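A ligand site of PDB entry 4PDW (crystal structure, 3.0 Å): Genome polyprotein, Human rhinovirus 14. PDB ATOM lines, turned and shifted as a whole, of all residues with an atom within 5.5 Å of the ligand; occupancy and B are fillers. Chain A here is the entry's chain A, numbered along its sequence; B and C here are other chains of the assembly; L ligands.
The side-chain hydroxyl (OH) of Tyr 128 lies close to an oxygen (O2) of the ligand (2.9 Å).
An oxygen (O4) of the ligand sits at hydrogen-bond distance from the side-chain hydroxyl of Tyr 152, 3.0 Å away.
O of Phe 186 lies within hydrogen-bond range of N of Tyr 128, at 2.8 Å.
The side-chain hydroxyl (OH) of Tyr 152 sits at hydrogen-bond distance from the backbone carbonyl oxygen (O) of Met 221 of chain A (2.8 Å).
The backbone NH of Tyr 152 is in hydrogen-bond range of the backbone carbonyl oxygen of Pro 174.
N of Val 191 lies within hydrogen-bond range of OH of Tyr 197 (3.3 Å).
The backbone carbonyl oxygen (O) of Ile 104 lies within hydrogen-bond range of the side-chain amide nitrogen (ND2) of Asn 219 (3.2 Å).
N of Val 188 is in hydrogen-bond range of O of Ser 126 (2.6 Å).
The side-chain hydroxyl (OG) of Ser 126 lies within hydrogen-bond range of a ring nitrogen (NE2) of His 245, at 2.9 Å.
The backbone NH (N) of Met 224 lies within hydrogen-bond range of the backbone carbonyl oxygen (O) of Trp 102 (2.9 Å).
CG2 of Ile 104 touches C9 of the ligand (3.5 Å).
Leu 106 touches the ligand.
OG of Ser 126 touches C2 of the ligand, 3.5 Å away.
Phe 186 touches the ligand.
CG1 of Val 188 touches O2 of the ligand, 3.8 Å away.
Val 191 touches the ligand.
Tyr 197 touches the ligand.
Met 221 of chain A touches the ligand (SD to C1, 3.9 Å).
Met 224 touches the ligand.
CD1 of Leu 221 of chain B touches O4 of the ligand (3.9 Å).
Leu 25 of chain C touches the ligand (CD1 to O4, 3.96 Å).
Hydrophobic or aromatic side chains within 4 Å of the ligand: Ile 104, Leu 106, Tyr 128, Tyr 152, Phe 186, Val 188, Val 191, Tyr 197, Met 221 of chain A, Met 224, Leu 221 of chain B and Leu 25 of chain C.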
ATOM      1  N   TRP A 102      12.875  21.025 -20.648  1.00  0.00           N
ATOM      2  CA  TRP A 102      13.220  20.499 -19.341  1.00  0.00           C
ATOM      3  C   TRP A 102      14.577  21.073 -19.014  1.00  0.00           C
ATOM      4  O   TRP A 102      15.580  20.699 -19.626  1.00  0.00           O
ATOM      5  CB  TRP A 102      13.292  18.968 -19.320  1.00  0.00           C
ATOM      6  CG  TRP A 102      13.818  18.451 -17.995  1.00  0.00           C
ATOM      7  CD1 TRP A 102      13.590  19.005 -16.759  1.00  0.00           C
ATOM      8  CD2 TRP A 102      14.667  17.322 -17.773  1.00  0.00           C
ATOM      9  NE1 TRP A 102      14.251  18.280 -15.779  1.00  0.00           N
ATOM     10  CE2 TRP A 102      14.916  17.248 -16.380  1.00  0.00           C
ATOM     11  CE3 TRP A 102      15.239  16.355 -18.615  1.00  0.00           C
ATOM     12  CZ2 TRP A 102      15.715  16.255 -15.809  1.00  0.00           C
ATOM     13  CZ3 TRP A 102      16.038  15.361 -18.044  1.00  0.00           C
ATOM     14  CH2 TRP A 102      16.264  15.321 -16.658  1.00  0.00           C
ATOM     15  N   ILE A 104      17.332  20.698 -17.297  1.00  0.00           N
ATOM     16  CA  ILE A 104      17.962  19.591 -16.576  1.00  0.00           C
ATOM     17  C   ILE A 104      18.346  19.947 -15.139  1.00  0.00           C
ATOM     18  O   ILE A 104      19.022  20.943 -14.894  1.00  0.00           O
ATOM     19  CB  ILE A 104      19.245  19.092 -17.271  1.00  0.00           C
ATOM     20  CG1 ILE A 104      19.061  19.043 -18.794  1.00  0.00           C
ATOM     21  CG2 ILE A 104      19.571  17.699 -16.767  1.00  0.00           C
ATOM     22  CD1 ILE A 104      18.132  17.975 -19.256  1.00  0.00           C
ATOM     23  N   LEU A 106      18.297  17.628 -10.971  1.00  0.00           N
ATOM     24  CA  LEU A 106      17.898  16.409 -10.283  1.00  0.00           C
ATOM     25  C   LEU A 106      17.180  16.632  -8.943  1.00  0.00           C
ATOM     26  O   LEU A 106      16.943  15.667  -8.206  1.00  0.00           O
ATOM     27  CB  LEU A 106      19.106  15.494 -10.071  1.00  0.00           C
ATOM     28  CG  LEU A 106      19.732  14.940 -11.353  1.00  0.00           C
ATOM     29  CD1 LEU A 106      20.923  14.069 -11.010  1.00  0.00           C
ATOM     30  CD2 LEU A 106      18.708  14.149 -12.130  1.00  0.00           C
ATOM     31  N   PHE A 124      29.677  11.011 -10.561  1.00  0.00           N
ATOM     32  CA  PHE A 124      29.223   9.779 -11.209  1.00  0.00           C
ATOM     33  C   PHE A 124      28.801   9.984 -12.659  1.00  0.00           C
ATOM     34  O   PHE A 124      28.608  11.120 -13.127  1.00  0.00           O
ATOM     35  CB  PHE A 124      28.049   9.183 -10.435  1.00  0.00           C
ATOM     36  CG  PHE A 124      26.894  10.136 -10.264  1.00  0.00           C
ATOM     37  CD1 PHE A 124      26.133  10.546 -11.360  1.00  0.00           C
ATOM     38  CD2 PHE A 124      26.562  10.653  -9.019  1.00  0.00           C
ATOM     39  CE1 PHE A 124      25.076  11.452 -11.216  1.00  0.00           C
ATOM     40  CE2 PHE A 124      25.509  11.562  -8.863  1.00  0.00           C
ATOM     41  CZ  PHE A 124      24.768  11.963  -9.955  1.00  0.00           C
ATOM     42  N   SER A 126      25.890   9.133 -15.576  1.00  0.00           N
ATOM     43  CA  SER A 126      24.449   8.978 -15.482  1.00  0.00           C
ATOM     44  C   SER A 126      23.884   8.138 -16.621  1.00  0.00           C
ATOM     45  O   SER A 126      24.305   8.256 -17.768  1.00  0.00           O
ATOM     46  CB  SER A 126      23.777  10.351 -15.476  1.00  0.00           C
ATOM     47  OG  SER A 126      24.315  11.203 -14.474  1.00  0.00           O
ATOM     48  N   TYR A 128      20.369   7.459 -18.365  1.00  0.00           N
ATOM     49  CA  TYR A 128      18.995   7.899 -18.481  1.00  0.00           C
ATOM     50  C   TYR A 128      18.113   6.896 -19.204  1.00  0.00           C
ATOM     51  O   TYR A 128      18.574   6.153 -20.074  1.00  0.00           O
ATOM     52  CB  TYR A 128      18.938   9.243 -19.199  1.00  0.00           C
ATOM     53  CG  TYR A 128      19.563  10.351 -18.404  1.00  0.00           C
ATOM     54  CD1 TYR A 128      18.870  10.979 -17.373  1.00  0.00           C
ATOM     55  CD2 TYR A 128      20.865  10.764 -18.667  1.00  0.00           C
ATOM     56  CE1 TYR A 128      19.467  11.987 -16.609  1.00  0.00           C
ATOM     57  CE2 TYR A 128      21.475  11.770 -17.922  1.00  0.00           C
ATOM     58  CZ  TYR A 128      20.771  12.377 -16.891  1.00  0.00           C
ATOM     59  OH  TYR A 128      21.404  13.349 -16.138  1.00  0.00           O
ATOM     60  N   ILE A 130      14.197   7.182 -20.791  1.00  0.00           N
ATOM     61  CA  ILE A 130      13.062   8.055 -21.016  1.00  0.00           C
ATOM     62  C   ILE A 130      11.857   7.280 -21.537  1.00  0.00           C
ATOM     63  O   ILE A 130      11.919   6.626 -22.574  1.00  0.00           O
ATOM     64  CB  ILE A 130      13.385   9.161 -22.042  1.00  0.00           C
ATOM     65  CG1 ILE A 130      14.682   9.864 -21.647  1.00  0.00           C
ATOM     66  CG2 ILE A 130      12.273  10.187 -22.065  1.00  0.00           C
ATOM     67  CD1 ILE A 130      15.118  10.895 -22.662  1.00  0.00           C
ATOM     68  N   TYR A 152      19.186  17.186 -26.736  1.00  0.00           N
ATOM     69  CA  TYR A 152      19.875  17.858 -25.646  1.00  0.00           C
ATOM     70  C   TYR A 152      20.383  19.199 -26.136  1.00  0.00           C
ATOM     71  O   TYR A 152      21.108  19.279 -27.119  1.00  0.00           O
ATOM     72  CB  TYR A 152      21.025  16.996 -25.126  1.00  0.00           C
ATOM     73  CG  TYR A 152      21.868  17.672 -24.082  1.00  0.00           C
ATOM     74  CD1 TYR A 152      21.296  18.226 -22.937  1.00  0.00           C
ATOM     75  CD2 TYR A 152      23.249  17.791 -24.241  1.00  0.00           C
ATOM     76  CE1 TYR A 152      22.067  18.885 -21.989  1.00  0.00           C
ATOM     77  CE2 TYR A 152      24.034  18.449 -23.289  1.00  0.00           C
ATOM     78  CZ  TYR A 152      23.430  18.991 -22.170  1.00  0.00           C
ATOM     79  OH  TYR A 152      24.198  19.647 -21.235  1.00  0.00           O
ATOM     80  N   PRO A 174      23.349  16.231 -29.299  1.00  0.00           N
ATOM     81  CA  PRO A 174      22.977  14.815 -29.430  1.00  0.00           C
ATOM     82  C   PRO A 174      21.470  14.716 -29.207  1.00  0.00           C
ATOM     83  O   PRO A 174      20.911  15.486 -28.427  1.00  0.00           O
ATOM     84  CB  PRO A 174      23.773  14.145 -28.299  1.00  0.00           C
ATOM     85  CG  PRO A 174      23.849  15.217 -27.254  1.00  0.00           C
ATOM     86  CD  PRO A 174      24.148  16.464 -28.076  1.00  0.00           C
ATOM     87  N   PHE A 186      20.292   5.632 -22.764  1.00  0.00           N
ATOM     88  CA  PHE A 186      21.674   5.985 -23.076  1.00  0.00           C
ATOM     89  C   PHE A 186      22.321   6.507 -21.807  1.00  0.00           C
ATOM     90  O   PHE A 186      21.635   6.883 -20.846  1.00  0.00           O
ATOM     91  CB  PHE A 186      21.708   7.084 -24.134  1.00  0.00           C
ATOM     92  CG  PHE A 186      20.968   8.325 -23.742  1.00  0.00           C
ATOM     93  CD1 PHE A 186      19.602   8.452 -24.015  1.00  0.00           C
ATOM     94  CD2 PHE A 186      21.621   9.359 -23.083  1.00  0.00           C
ATOM     95  CE1 PHE A 186      18.913   9.593 -23.640  1.00  0.00           C
ATOM     96  CE2 PHE A 186      20.931  10.500 -22.708  1.00  0.00           C
ATOM     97  CZ  PHE A 186      19.572  10.619 -22.982  1.00  0.00           C
ATOM     98  N   VAL A 188      25.443   9.082 -19.979  1.00  0.00           N
ATOM     99  CA  VAL A 188      26.161  10.335 -20.153  1.00  0.00           C
ATOM    100  C   VAL A 188      27.315  10.370 -19.156  1.00  0.00           C
ATOM    101  O   VAL A 188      27.122  10.089 -17.977  1.00  0.00           O
ATOM    102  CB  VAL A 188      25.242  11.534 -19.856  1.00  0.00           C
ATOM    103  CG1 VAL A 188      25.970  12.840 -20.120  1.00  0.00           C
ATOM    104  CG2 VAL A 188      23.984  11.428 -20.702  1.00  0.00           C
ATOM    105  N   PRO A 189      28.516  10.721 -19.616  1.00  0.00           N
ATOM    106  CA  PRO A 189      29.670  10.788 -18.708  1.00  0.00           C
ATOM    107  C   PRO A 189      29.507  11.923 -17.709  1.00  0.00           C
ATOM    108  O   PRO A 189      28.658  12.786 -17.877  1.00  0.00           O
ATOM    109  CB  PRO A 189      30.831  11.027 -19.661  1.00  0.00           C
ATOM    110  CG  PRO A 189      30.191  11.867 -20.738  1.00  0.00           C
ATOM    111  CD  PRO A 189      28.897  11.133 -20.977  1.00  0.00           C
ATOM    112  N   VAL A 191      29.627  15.165 -16.423  1.00  0.00           N
ATOM    113  CA  VAL A 191      29.821  16.445 -17.091  1.00  0.00           C
ATOM    114  C   VAL A 191      30.101  17.662 -16.229  1.00  0.00           C
ATOM    115  O   VAL A 191      30.133  18.782 -16.740  1.00  0.00           O
ATOM    116  CB  VAL A 191      28.634  16.797 -17.993  1.00  0.00           C
ATOM    117  CG1 VAL A 191      28.644  15.926 -19.240  1.00  0.00           C
ATOM    118  CG2 VAL A 191      27.336  16.608 -17.212  1.00  0.00           C
ATOM    119  N   TYR A 197      30.156  17.078  -8.457  1.00  0.00           N
ATOM    120  CA  TYR A 197      28.961  17.917  -8.492  1.00  0.00           C
ATOM    121  C   TYR A 197      28.742  18.401  -7.056  1.00  0.00           C
ATOM    122  O   TYR A 197      29.116  17.721  -6.089  1.00  0.00           O
ATOM    123  CB  TYR A 197      27.725  17.122  -8.909  1.00  0.00           C
ATOM    124  CG  TYR A 197      27.697  16.543 -10.303  1.00  0.00           C
ATOM    125  CD1 TYR A 197      27.815  17.348 -11.431  1.00  0.00           C
ATOM    126  CD2 TYR A 197      27.460  15.180 -10.493  1.00  0.00           C
ATOM    127  CE1 TYR A 197      27.684  16.820 -12.721  1.00  0.00           C
ATOM    128  CE2 TYR A 197      27.325  14.635 -11.779  1.00  0.00           C
ATOM    129  CZ  TYR A 197      27.438  15.462 -12.880  1.00  0.00           C
ATOM    130  OH  TYR A 197      27.301  14.900 -14.139  1.00  0.00           O
ATOM    131  N   ASN A 198      28.139  19.575  -6.895  1.00  0.00           N
ATOM    132  CA  ASN A 198      27.855  20.116  -5.571  1.00  0.00           C
ATOM    133  C   ASN A 198      26.392  19.865  -5.263  1.00  0.00           C
ATOM    134  O   ASN A 198      25.517  20.151  -6.094  1.00  0.00           O
ATOM    135  CB  ASN A 198      28.096  21.620  -5.509  1.00  0.00           C
ATOM    136  CG  ASN A 198      29.553  21.973  -5.377  1.00  0.00           C
ATOM    137  OD1 ASN A 198      30.393  21.481  -6.127  1.00  0.00           O
ATOM    138  ND2 ASN A 198      29.876  22.842  -4.419  1.00  0.00           N
ATOM    139  N   ASN A 219      24.146  25.017 -11.181  1.00  0.00           N
ATOM    140  CA  ASN A 219      23.396  24.122 -12.035  1.00  0.00           C
ATOM    141  C   ASN A 219      22.816  24.683 -13.329  1.00  0.00           C
ATOM    142  O   ASN A 219      21.596  24.769 -13.480  1.00  0.00           O
ATOM    143  CB  ASN A 219      22.270  23.449 -11.260  1.00  0.00           C
ATOM    144  CG  ASN A 219      21.571  22.358 -12.073  1.00  0.00           C
ATOM    145  OD1 ASN A 219      22.111  21.250 -12.244  1.00  0.00           O
ATOM    146  ND2 ASN A 219      20.388  22.680 -12.608  1.00  0.00           N
ATOM    147  N   MET A 221      22.949  23.365 -16.519  1.00  0.00           N
ATOM    148  CA  MET A 221      23.202  22.179 -17.339  1.00  0.00           C
ATOM    149  C   MET A 221      22.526  22.175 -18.699  1.00  0.00           C
ATOM    150  O   MET A 221      22.701  21.235 -19.463  1.00  0.00           O
ATOM    151  CB  MET A 221      22.748  20.923 -16.604  1.00  0.00           C
ATOM    152  CG  MET A 221      23.318  20.743 -15.219  1.00  0.00           C
ATOM    153  SD  MET A 221      25.100  20.605 -15.243  1.00  0.00           S
ATOM    154  CE  MET A 221      25.551  22.085 -14.336  1.00  0.00           C
ATOM    155  N   MET A 224      16.586  19.897 -22.269  1.00  0.00           N
ATOM    156  CA  MET A 224      16.300  18.737 -23.081  1.00  0.00           C
ATOM    157  C   MET A 224      14.991  19.131 -23.765  1.00  0.00           C
ATOM    158  O   MET A 224      13.974  19.359 -23.095  1.00  0.00           O
ATOM    159  CB  MET A 224      16.079  17.503 -22.218  1.00  0.00           C
ATOM    160  CG  MET A 224      15.735  16.253 -23.024  1.00  0.00           C
ATOM    161  SD  MET A 224      17.164  15.258 -23.428  1.00  0.00           S
ATOM    162  CE  MET A 224      16.721  13.772 -22.633  1.00  0.00           C
ATOM    163  N   HIS A 245      16.691   8.490 -13.939  1.00  0.00           N
ATOM    164  CA  HIS A 245      18.137   8.623 -13.774  1.00  0.00           C
ATOM    165  C   HIS A 245      18.762   7.580 -12.846  1.00  0.00           C
ATOM    166  O   HIS A 245      18.294   7.370 -11.733  1.00  0.00           O
ATOM    167  CB  HIS A 245      18.475  10.027 -13.261  1.00  0.00           C
ATOM    168  CG  HIS A 245      19.917  10.208 -12.871  1.00  0.00           C
ATOM    169  ND1 HIS A 245      20.477   9.600 -11.764  1.00  0.00           N
ATOM    170  CD2 HIS A 245      20.904  10.923 -13.446  1.00  0.00           C
ATOM    171  CE1 HIS A 245      21.753   9.934 -11.686  1.00  0.00           C
ATOM    172  NE2 HIS A 245      22.044  10.736 -12.693  1.00  0.00           N
ATOM    173  N   LEU B 221      32.253  18.786 -24.753  1.00  0.00           N
ATOM    174  CA  LEU B 221      30.818  18.666 -24.977  1.00  0.00           C
ATOM    175  C   LEU B 221      30.332  19.410 -26.202  1.00  0.00           C
ATOM    176  O   LEU B 221      29.838  20.536 -26.110  1.00  0.00           O
ATOM    177  CB  LEU B 221      30.058  19.148 -23.730  1.00  0.00           C
ATOM    178  CG  LEU B 221      28.802  18.361 -23.367  1.00  0.00           C
ATOM    179  CD1 LEU B 221      28.300  18.793 -22.007  1.00  0.00           C
ATOM    180  CD2 LEU B 221      27.747  18.558 -24.442  1.00  0.00           C
ATOM    181  N   ALA C  24      25.910   9.129 -24.922  1.00  0.00           N
ATOM    182  CA  ALA C  24      25.380  10.196 -25.755  1.00  0.00           C
ATOM    183  C   ALA C  24      26.435  11.256 -26.060  1.00  0.00           C
ATOM    184  O   ALA C  24      26.253  12.070 -26.963  1.00  0.00           O
ATOM    185  CB  ALA C  24      24.182  10.835 -25.085  1.00  0.00           C
ATOM    186  N   LEU C  25      27.542  11.238 -25.317  1.00  0.00           N
ATOM    187  CA  LEU C  25      28.630  12.189 -25.504  1.00  0.00           C
ATOM    188  C   LEU C  25      29.936  11.434 -25.747  1.00  0.00           C
ATOM    189  O   LEU C  25      30.791  11.326 -24.862  1.00  0.00           O
ATOM    190  CB  LEU C  25      28.797  13.079 -24.269  1.00  0.00           C
ATOM    191  CG  LEU C  25      27.585  13.832 -23.731  1.00  0.00           C
ATOM    192  CD1 LEU C  25      28.015  14.701 -22.571  1.00  0.00           C
ATOM    193  CD2 LEU C  25      26.972  14.696 -24.814  1.00  0.00           C
HETATM  194  C1  LIG L   1      24.148  17.231 -13.567  1.00  0.00           C
HETATM  195  C2  LIG L   1      23.558  14.598 -14.286  1.00  0.00           C
HETATM  196  C3  LIG L   1      23.230  15.852 -20.025  1.00  0.00           C
HETATM  197  C4  LIG L   1      22.731  14.234 -23.511  1.00  0.00           C
HETATM  198  C5  LIG L   1      19.626  12.386 -20.763  1.00  0.00           C
HETATM  199  O1  LIG L   1      19.543  13.765 -20.584  1.00  0.00           O
HETATM  200  C6  LIG L   1      20.816  14.446 -20.403  1.00  0.00           C
HETATM  201  C7  LIG L   1      21.082  14.910 -19.200  1.00  0.00           C
HETATM  202  C8  LIG L   1      22.335  15.637 -18.978  1.00  0.00           C
HETATM  203  C9  LIG L   1      22.610  16.215 -17.568  1.00  0.00           C
HETATM  204  C10 LIG L   1      23.500  15.208 -16.751  1.00  0.00           C
HETATM  205  C11 LIG L   1      23.651  15.571 -15.245  1.00  0.00           C
HETATM  206  C12 LIG L   1      23.939  16.902 -14.905  1.00  0.00           C
HETATM  207  C13 LIG L   1      24.058  16.248 -12.600  1.00  0.00           C
HETATM  208  C14 LIG L   1      24.285  16.601 -11.182  1.00  0.00           C
HETATM  209  N1  LIG L   1      24.363  16.886 -10.112  1.00  0.00           N
HETATM  210  C15 LIG L   1      23.774  14.933 -12.944  1.00  0.00           C
HETATM  211  O2  LIG L   1      23.994  14.218 -17.173  1.00  0.00           O
HETATM  212  C16 LIG L   1      22.959  15.359 -21.273  1.00  0.00           C
HETATM  213  C17 LIG L   1      21.743  14.650 -21.488  1.00  0.00           C
HETATM  214  O3  LIG L   1      21.516  14.236 -22.750  1.00  0.00           O
HETATM  215  N2  LIG L   1      24.451  16.670 -19.827  1.00  0.00           N
HETATM  216  O4  LIG L   1      25.189  16.826 -20.791  1.00  0.00           O
HETATM  217  O5  LIG L   1      24.724  17.188 -18.758  1.00  0.00           O
